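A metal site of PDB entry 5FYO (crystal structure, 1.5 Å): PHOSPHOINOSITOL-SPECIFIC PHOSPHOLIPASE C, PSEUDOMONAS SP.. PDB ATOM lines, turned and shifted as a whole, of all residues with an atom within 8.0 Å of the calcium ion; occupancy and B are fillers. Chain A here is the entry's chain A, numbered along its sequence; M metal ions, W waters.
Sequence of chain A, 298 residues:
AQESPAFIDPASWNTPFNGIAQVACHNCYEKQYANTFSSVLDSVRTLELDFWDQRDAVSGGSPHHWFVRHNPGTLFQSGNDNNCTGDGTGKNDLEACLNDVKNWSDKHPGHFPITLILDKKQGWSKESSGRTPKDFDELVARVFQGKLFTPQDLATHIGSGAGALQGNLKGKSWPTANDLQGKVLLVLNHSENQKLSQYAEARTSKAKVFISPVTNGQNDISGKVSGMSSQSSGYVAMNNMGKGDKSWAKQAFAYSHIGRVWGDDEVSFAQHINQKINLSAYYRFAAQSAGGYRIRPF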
ATOM      1  N   CYS A  25     -22.693  15.810 -17.770  1.00  0.00           N
ATOM      2  CA  CYS A  25     -21.367  15.293 -17.995  1.00  0.00           C
ATOM      3  C   CYS A  25     -21.426  13.978 -18.766  1.00  0.00           C
ATOM      4  O   CYS A  25     -22.470  13.339 -18.855  1.00  0.00           O
ATOM      5  CB  CYS A  25     -20.596  15.123 -16.685  1.00  0.00           C
ATOM      6  SG  CYS A  25     -20.808  13.516 -15.858  1.00  0.00           S
ATOM      7  N   HIS A  26     -20.271  13.548 -19.261  1.00  0.00           N
ATOM      8  CA  HIS A  26     -20.102  12.181 -19.732  1.00  0.00           C
ATOM      9  C   HIS A  26     -18.885  11.655 -18.951  1.00  0.00           C
ATOM     10  O   HIS A  26     -17.759  12.120 -19.176  1.00  0.00           O
ATOM     11  CB  HIS A  26     -19.916  12.133 -21.262  1.00  0.00           C
ATOM     12  CG  HIS A  26     -19.954  10.750 -21.843  1.00  0.00           C
ATOM     13  ND1 HIS A  26     -19.940  10.496 -23.196  1.00  0.00           N
ATOM     14  CD2 HIS A  26     -20.080   9.549 -21.252  1.00  0.00           C
ATOM     15  CE1 HIS A  26     -19.962   9.193 -23.396  1.00  0.00           C
ATOM     16  NE2 HIS A  26     -20.049   8.598 -22.229  1.00  0.00           N
ATOM     17  N   ASN A  27     -19.109  10.651 -18.085  1.00  0.00           N
ATOM     18  CA  ASN A  27     -18.015   9.972 -17.391  1.00  0.00           C
ATOM     19  C   ASN A  27     -17.163  10.934 -16.577  1.00  0.00           C
ATOM     20  O   ASN A  27     -15.930  10.783 -16.456  1.00  0.00           O
ATOM     21  CB  ASN A  27     -17.145   9.141 -18.345  1.00  0.00           C
ATOM     22  CG  ASN A  27     -17.892   7.952 -18.955  1.00  0.00           C
ATOM     23  OD1 ASN A  27     -18.926   7.530 -18.459  1.00  0.00           O
ATOM     24  ND2 ASN A  27     -17.366   7.411 -20.063  1.00  0.00           N
ATOM     25  N   CYS A  28     -17.828  11.870 -15.895  1.00  0.00           N
ATOM     26  CA  CYS A  28     -17.110  12.926 -15.180  1.00  0.00           C
ATOM     27  C   CYS A  28     -16.435  12.462 -13.880  1.00  0.00           C
ATOM     28  O   CYS A  28     -15.745  13.236 -13.223  1.00  0.00           O
ATOM     29  CB  CYS A  28     -17.942  14.160 -14.898  1.00  0.00           C
ATOM     30  SG  CYS A  28     -19.453  13.796 -14.045  1.00  0.00           S
ATOM     31  N   TYR A  29     -16.632  11.197 -13.506  1.00  0.00           N
ATOM     32  CA  TYR A  29     -15.875  10.551 -12.442  1.00  0.00           C
ATOM     33  C   TYR A  29     -14.408  10.320 -12.828  1.00  0.00           C
ATOM     34  O   TYR A  29     -13.594  10.067 -11.946  1.00  0.00           O
ATOM     35  CB  TYR A  29     -16.535   9.200 -12.035  1.00  0.00           C
ATOM     36  CG  TYR A  29     -16.341   8.180 -13.094  1.00  0.00           C
ATOM     37  CD1 TYR A  29     -15.190   7.365 -13.148  1.00  0.00           C
ATOM     38  CD2 TYR A  29     -17.296   8.018 -14.113  1.00  0.00           C
ATOM     39  CE1 TYR A  29     -14.984   6.487 -14.193  1.00  0.00           C
ATOM     40  CE2 TYR A  29     -17.081   7.126 -15.156  1.00  0.00           C
ATOM     41  CZ  TYR A  29     -15.934   6.346 -15.175  1.00  0.00           C
ATOM     42  OH  TYR A  29     -15.696   5.474 -16.237  1.00  0.00           O
ATOM     43  N   GLU A  30     -14.052  10.418 -14.114  1.00  0.00           N
ATOM     44  CA  GLU A  30     -12.679  10.217 -14.544  1.00  0.00           C
ATOM     45  C   GLU A  30     -11.822  11.464 -14.254  1.00  0.00           C
ATOM     46  O   GLU A  30     -12.260  12.597 -14.527  1.00  0.00           O
ATOM     47  CB  GLU A  30     -12.587   9.868 -16.034  1.00  0.00           C
ATOM     48  CG  GLU A  30     -13.298   8.581 -16.422  1.00  0.00           C
ATOM     49  CD  GLU A  30     -12.976   8.135 -17.842  1.00  0.00           C
ATOM     50  OE1 GLU A  30     -11.800   7.826 -18.113  1.00  0.00           O
ATOM     51  OE2 GLU A  30     -13.919   8.016 -18.659  1.00  0.00           O
ATOM     52  N   GLU A  48     -22.326  11.410 -13.739  1.00  0.00           N
ATOM     53  CA  GLU A  48     -22.289   9.998 -14.151  1.00  0.00           C
ATOM     54  C   GLU A  48     -21.216   9.228 -13.395  1.00  0.00           C
ATOM     55  O   GLU A  48     -20.122   9.768 -13.183  1.00  0.00           O
ATOM     56  CB  GLU A  48     -21.996   9.877 -15.665  1.00  0.00           C
ATOM     57  CG  GLU A  48     -21.944   8.428 -16.181  1.00  0.00           C
ATOM     58  CD  GLU A  48     -21.953   8.343 -17.697  1.00  0.00           C
ATOM     59  OE1 GLU A  48     -21.716   9.413 -18.369  1.00  0.00           O
ATOM     60  OE2 GLU A  48     -22.179   7.205 -18.194  1.00  0.00           O
ATOM     61  N   LEU A  49     -21.544   7.988 -13.020  1.00  0.00           N
ATOM     62  CA  LEU A  49     -20.616   7.036 -12.412  1.00  0.00           C
ATOM     63  C   LEU A  49     -20.713   5.695 -13.131  1.00  0.00           C
ATOM     64  O   LEU A  49     -21.834   5.177 -13.297  1.00  0.00           O
ATOM     65  CB  LEU A  49     -21.024   6.813 -10.933  1.00  0.00           C
ATOM     66  CG  LEU A  49     -20.803   8.019 -10.044  1.00  0.00           C
ATOM     67  CD1 LEU A  49     -21.628   7.938  -8.793  1.00  0.00           C
ATOM     68  CD2 LEU A  49     -19.309   8.189  -9.731  1.00  0.00           C
ATOM     69  N   ASP A  50     -19.567   5.132 -13.518  1.00  0.00           N
ATOM     70  CA  ASP A  50     -19.474   3.773 -14.094  1.00  0.00           C
ATOM     71  C   ASP A  50     -19.101   2.855 -12.940  1.00  0.00           C
ATOM     72  O   ASP A  50     -18.113   3.091 -12.267  1.00  0.00           O
ATOM     73  CB  ASP A  50     -18.396   3.672 -15.169  1.00  0.00           C
ATOM     74  CG  ASP A  50     -18.732   4.418 -16.459  1.00  0.00           C
ATOM     75  OD1 ASP A  50     -19.886   4.855 -16.650  1.00  0.00           O
ATOM     76  OD2 ASP A  50     -17.789   4.534 -17.271  1.00  0.00           O
ATOM     77  N   PHE A  51     -19.898   1.802 -12.715  1.00  0.00           N
ATOM     78  CA  PHE A  51     -19.709   0.974 -11.532  1.00  0.00           C
ATOM     79  C   PHE A  51     -19.651  -0.509 -11.825  1.00  0.00           C
ATOM     80  O   PHE A  51     -20.405  -1.035 -12.617  1.00  0.00           O
ATOM     81  CB  PHE A  51     -20.718   1.350 -10.400  1.00  0.00           C
ATOM     82  CG  PHE A  51     -22.134   0.860 -10.618  1.00  0.00           C
ATOM     83  CD1 PHE A  51     -23.051   1.583 -11.407  1.00  0.00           C
ATOM     84  CD2 PHE A  51     -22.592  -0.275  -9.963  1.00  0.00           C
ATOM     85  CE1 PHE A  51     -24.343   1.141 -11.557  1.00  0.00           C
ATOM     86  CE2 PHE A  51     -23.892  -0.725 -10.136  1.00  0.00           C
ATOM     87  CZ  PHE A  51     -24.780  -0.030 -10.920  1.00  0.00           C
ATOM     88  N   ARG A  69     -14.795   2.862 -11.836  1.00  0.00           N
ATOM     89  CA  ARG A  69     -13.691   2.995 -12.775  1.00  0.00           C
ATOM     90  C   ARG A  69     -14.225   2.825 -14.181  1.00  0.00           C
ATOM     91  O   ARG A  69     -15.351   2.364 -14.364  1.00  0.00           O
ATOM     92  CB  ARG A  69     -12.589   1.922 -12.540  1.00  0.00           C
ATOM     93  CG  ARG A  69     -13.052   0.474 -12.789  1.00  0.00           C
ATOM     94  CD  ARG A  69     -11.919  -0.536 -12.615  1.00  0.00           C
ATOM     95  NE  ARG A  69     -12.352  -1.900 -12.918  1.00  0.00           N
ATOM     96  CZ  ARG A  69     -12.984  -2.697 -12.058  1.00  0.00           C
ATOM     97  NH1 ARG A  69     -13.204  -2.325 -10.794  1.00  0.00           N
ATOM     98  NH2 ARG A  69     -13.413  -3.878 -12.492  1.00  0.00           N
ATOM     99  N   HIS A  70     -13.410   3.177 -15.181  1.00  0.00           N
ATOM    100  CA  HIS A  70     -13.831   3.075 -16.586  1.00  0.00           C
ATOM    101  C   HIS A  70     -13.617   1.664 -17.164  1.00  0.00           C
ATOM    102  O   HIS A  70     -14.517   1.115 -17.791  1.00  0.00           O
ATOM    103  CB  HIS A  70     -13.124   4.103 -17.431  1.00  0.00           C
ATOM    104  CG  HIS A  70     -13.674   4.217 -18.815  1.00  0.00           C
ATOM    105  ND1 HIS A  70     -13.168   3.522 -19.882  1.00  0.00           N
ATOM    106  CD2 HIS A  70     -14.697   4.953 -19.299  1.00  0.00           C
ATOM    107  CE1 HIS A  70     -13.859   3.819 -20.968  1.00  0.00           C
ATOM    108  NE2 HIS A  70     -14.775   4.702 -20.651  1.00  0.00           N
ATOM    109  N   ILE A 117     -26.474   9.511 -13.286  1.00  0.00           N
ATOM    110  CA  ILE A 117     -26.487   8.371 -14.202  1.00  0.00           C
ATOM    111  C   ILE A 117     -25.524   7.298 -13.637  1.00  0.00           C
ATOM    112  O   ILE A 117     -24.339   7.538 -13.479  1.00  0.00           O
ATOM    113  CB  ILE A 117     -26.033   8.806 -15.620  1.00  0.00           C
ATOM    114  CG1 ILE A 117     -26.858  10.024 -16.131  1.00  0.00           C
ATOM    115  CG2 ILE A 117     -26.054   7.637 -16.552  1.00  0.00           C
ATOM    116  CD1 ILE A 117     -28.349   9.842 -16.199  1.00  0.00           C
ATOM    117  N   LEU A 118     -26.091   6.156 -13.277  1.00  0.00           N
ATOM    118  CA  LEU A 118     -25.358   5.053 -12.739  1.00  0.00           C
ATOM    119  C   LEU A 118     -25.251   4.000 -13.832  1.00  0.00           C
ATOM    120  O   LEU A 118     -26.201   3.236 -14.098  1.00  0.00           O
ATOM    121  CB  LEU A 118     -26.065   4.538 -11.472  1.00  0.00           C
ATOM    122  CG  LEU A 118     -26.300   5.594 -10.398  1.00  0.00           C
ATOM    123  CD1 LEU A 118     -27.122   5.039  -9.248  1.00  0.00           C
ATOM    124  CD2 LEU A 118     -25.014   6.238  -9.894  1.00  0.00           C
ATOM    125  N   ASP A 119     -24.075   3.985 -14.465  1.00  0.00           N
ATOM    126  CA  ASP A 119     -23.836   3.161 -15.663  1.00  0.00           C
ATOM    127  C   ASP A 119     -23.192   1.855 -15.171  1.00  0.00           C
ATOM    128  O   ASP A 119     -21.985   1.778 -14.869  1.00  0.00           O
ATOM    129  CB  ASP A 119     -22.934   3.936 -16.640  1.00  0.00           C
ATOM    130  CG  ASP A 119     -22.825   3.276 -18.023  1.00  0.00           C
ATOM    131  OD1 ASP A 119     -23.491   2.244 -18.266  1.00  0.00           O
ATOM    132  OD2 ASP A 119     -22.022   3.821 -18.848  1.00  0.00           O
ATOM    133  N   LYS A 120     -24.025   0.830 -15.109  1.00  0.00           N
ATOM    134  CA  LYS A 120     -23.620  -0.455 -14.567  1.00  0.00           C
ATOM    135  C   LYS A 120     -22.825  -1.228 -15.619  1.00  0.00           C
ATOM    136  O   LYS A 120     -23.263  -1.327 -16.769  1.00  0.00           O
ATOM    137  CB  LYS A 120     -24.853  -1.248 -14.161  1.00  0.00           C
ATOM    138  CG  LYS A 120     -24.527  -2.501 -13.359  1.00  0.00           C
ATOM    139  CD  LYS A 120     -25.756  -3.236 -12.896  1.00  0.00           C
ATOM    140  CE  LYS A 120     -25.516  -4.172 -11.739  1.00  0.00           C
ATOM    141  NZ  LYS A 120     -24.265  -4.917 -11.637  1.00  0.00           N
ATOM    142  N   LYS A 121     -21.710  -1.818 -15.188  1.00  0.00           N
ATOM    143  CA  LYS A 121     -20.794  -2.466 -16.151  1.00  0.00           C
ATOM    144  C   LYS A 121     -20.752  -3.988 -16.132  1.00  0.00           C
ATOM    145  O   LYS A 121     -20.215  -4.583 -17.052  1.00  0.00           O
ATOM    146  CB  LYS A 121     -19.371  -1.900 -15.969  1.00  0.00           C
ATOM    147  CG  LYS A 121     -19.276  -0.419 -16.232  1.00  0.00           C
ATOM    148  CD  LYS A 121     -19.564  -0.122 -17.716  1.00  0.00           C
ATOM    149  CE  LYS A 121     -19.747   1.366 -17.949  1.00  0.00           C
ATOM    150  NZ  LYS A 121     -19.993   1.677 -19.369  1.00  0.00           N
ATOM    151  N   ASN A 189     -28.252   2.795 -16.149  1.00  0.00           N
ATOM    152  CA  ASN A 189     -27.933   2.434 -17.541  1.00  0.00           C
ATOM    153  C   ASN A 189     -27.114   1.126 -17.545  1.00  0.00           C
ATOM    154  O   ASN A 189     -26.527   0.739 -16.523  1.00  0.00           O
ATOM    155  CB  ASN A 189     -27.062   3.502 -18.191  1.00  0.00           C
ATOM    156  CG  ASN A 189     -27.780   4.812 -18.522  1.00  0.00           C
ATOM    157  OD1 ASN A 189     -29.017   5.036 -18.329  1.00  0.00           O
ATOM    158  ND2 ASN A 189     -26.996   5.700 -19.025  1.00  0.00           N
ATOM    159  N   ARG A 260     -31.651  11.061 -22.632  1.00  0.00           N
ATOM    160  CA  ARG A 260     -30.238  11.393 -22.556  1.00  0.00           C
ATOM    161  C   ARG A 260     -29.590  10.968 -23.855  1.00  0.00           C
ATOM    162  O   ARG A 260     -29.795   9.845 -24.292  1.00  0.00           O
ATOM    163  CB  ARG A 260     -29.561  10.680 -21.374  1.00  0.00           C
ATOM    164  CG  ARG A 260     -28.086  11.047 -21.238  1.00  0.00           C
ATOM    165  CD  ARG A 260     -27.653  10.795 -19.769  1.00  0.00           C
ATOM    166  NE  ARG A 260     -26.241  11.052 -19.499  1.00  0.00           N
ATOM    167  CZ  ARG A 260     -25.262  10.239 -19.822  1.00  0.00           C
ATOM    168  NH1 ARG A 260     -25.512   9.121 -20.502  1.00  0.00           N
ATOM    169  NH2 ARG A 260     -24.003  10.564 -19.467  1.00  0.00           N
ATOM    170  N   TRP A 262     -25.730  10.649 -25.516  1.00  0.00           N
ATOM    171  CA  TRP A 262     -24.267  10.664 -25.292  1.00  0.00           C
ATOM    172  C   TRP A 262     -23.521  10.441 -26.601  1.00  0.00           C
ATOM    173  O   TRP A 262     -24.049   9.880 -27.558  1.00  0.00           O
ATOM    174  CB  TRP A 262     -23.853   9.616 -24.230  1.00  0.00           C
ATOM    175  CG  TRP A 262     -24.265   8.194 -24.615  1.00  0.00           C
ATOM    176  CD1 TRP A 262     -25.468   7.584 -24.307  1.00  0.00           C
ATOM    177  CD2 TRP A 262     -23.499   7.248 -25.361  1.00  0.00           C
ATOM    178  NE1 TRP A 262     -25.481   6.327 -24.828  1.00  0.00           N
ATOM    179  CE2 TRP A 262     -24.280   6.079 -25.461  1.00  0.00           C
ATOM    180  CE3 TRP A 262     -22.208   7.239 -25.884  1.00  0.00           C
ATOM    181  CZ2 TRP A 262     -23.843   4.943 -26.139  1.00  0.00           C
ATOM    182  CZ3 TRP A 262     -21.758   6.103 -26.574  1.00  0.00           C
ATOM    183  CH2 TRP A 262     -22.579   4.970 -26.674  1.00  0.00           C
ATOM    184  N   TYR A 283     -18.230  15.205 -22.583  1.00  0.00           N
ATOM    185  CA  TYR A 283     -16.991  15.032 -21.832  1.00  0.00           C
ATOM    186  C   TYR A 283     -16.523  16.390 -21.287  1.00  0.00           C
ATOM    187  O   TYR A 283     -16.170  16.520 -20.107  1.00  0.00           O
ATOM    188  CB  TYR A 283     -15.902  14.430 -22.720  1.00  0.00           C
ATOM    189  CG  TYR A 283     -16.167  13.010 -23.206  1.00  0.00           C
ATOM    190  CD1 TYR A 283     -16.194  11.951 -22.316  1.00  0.00           C
ATOM    191  CD2 TYR A 283     -16.431  12.728 -24.535  1.00  0.00           C
ATOM    192  CE1 TYR A 283     -16.425  10.666 -22.734  1.00  0.00           C
ATOM    193  CE2 TYR A 283     -16.658  11.421 -24.987  1.00  0.00           C
ATOM    194  CZ  TYR A 283     -16.650  10.383 -24.057  1.00  0.00           C
ATOM    195  OH  TYR A 283     -16.890   9.084 -24.419  1.00  0.00           O
HETATM  196 CA    CA M   1     -20.501   5.707 -18.704  1.00  0.00          CA
HETATM  197  O   HOH W   1     -18.790   4.528 -19.858  1.00  0.00           O
HETATM  198  O   HOH W   2     -21.172   6.041 -21.139  1.00  0.00           O
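Water W1 lies within hydrogen-bond range of the side-chain carboxylate of Asp 50 (2.8 Å), the side-chain amino group of Lys 121 (3.1 Å) and the side-chain amide nitrogen of Asn 27 (3.2 Å).
The side-chain carboxylate (OD1) of Asp 119 is in salt-bridge range of the side-chain amino group (NZ) of Lys 121 (3.7 Å).
The backbone carbonyl oxygen of Asp 119 is in hydrogen-bond range of the backbone NH of Phe 51 (3.0 Å).
N of Glu 48 sits at hydrogen-bond distance from SG of Cys 28, 3.7 Å away.
The backbone NH of Arg 69 sits at hydrogen-bond distance from the backbone carbonyl oxygen of Asp 50, 3.4 Å away.
OD2 of Asp 50 is in hydrogen-bond range of OH of Tyr 29 (2.5 Å).
The backbone NH (N) of Glu 48 sits at hydrogen-bond distance from the side-chain sulfur (SG) of Cys 25 (3.4 Å).
SG of Cys 28 forms a disulfide with SG of Cys 25, at 2.3 Å.
OE1 of Glu 48 lies within salt-bridge range of NH2 of Arg 260, 2.8 Å away.
OE2 of Glu 48 is bound to the calcium ion (2.3 Å).
The side-chain carboxylate (OD1) of Asp 50 is bound to the calcium ion (2.3 Å).
Water W1 binds the calcium ion, 2.4 Å away.
OD1 of Asn 27 binds the calcium ion, 2.4 Å away.
OD2 of Asp 119 is bound to the calcium ion.
Water W2 binds the calcium ion, at 2.5 Å.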
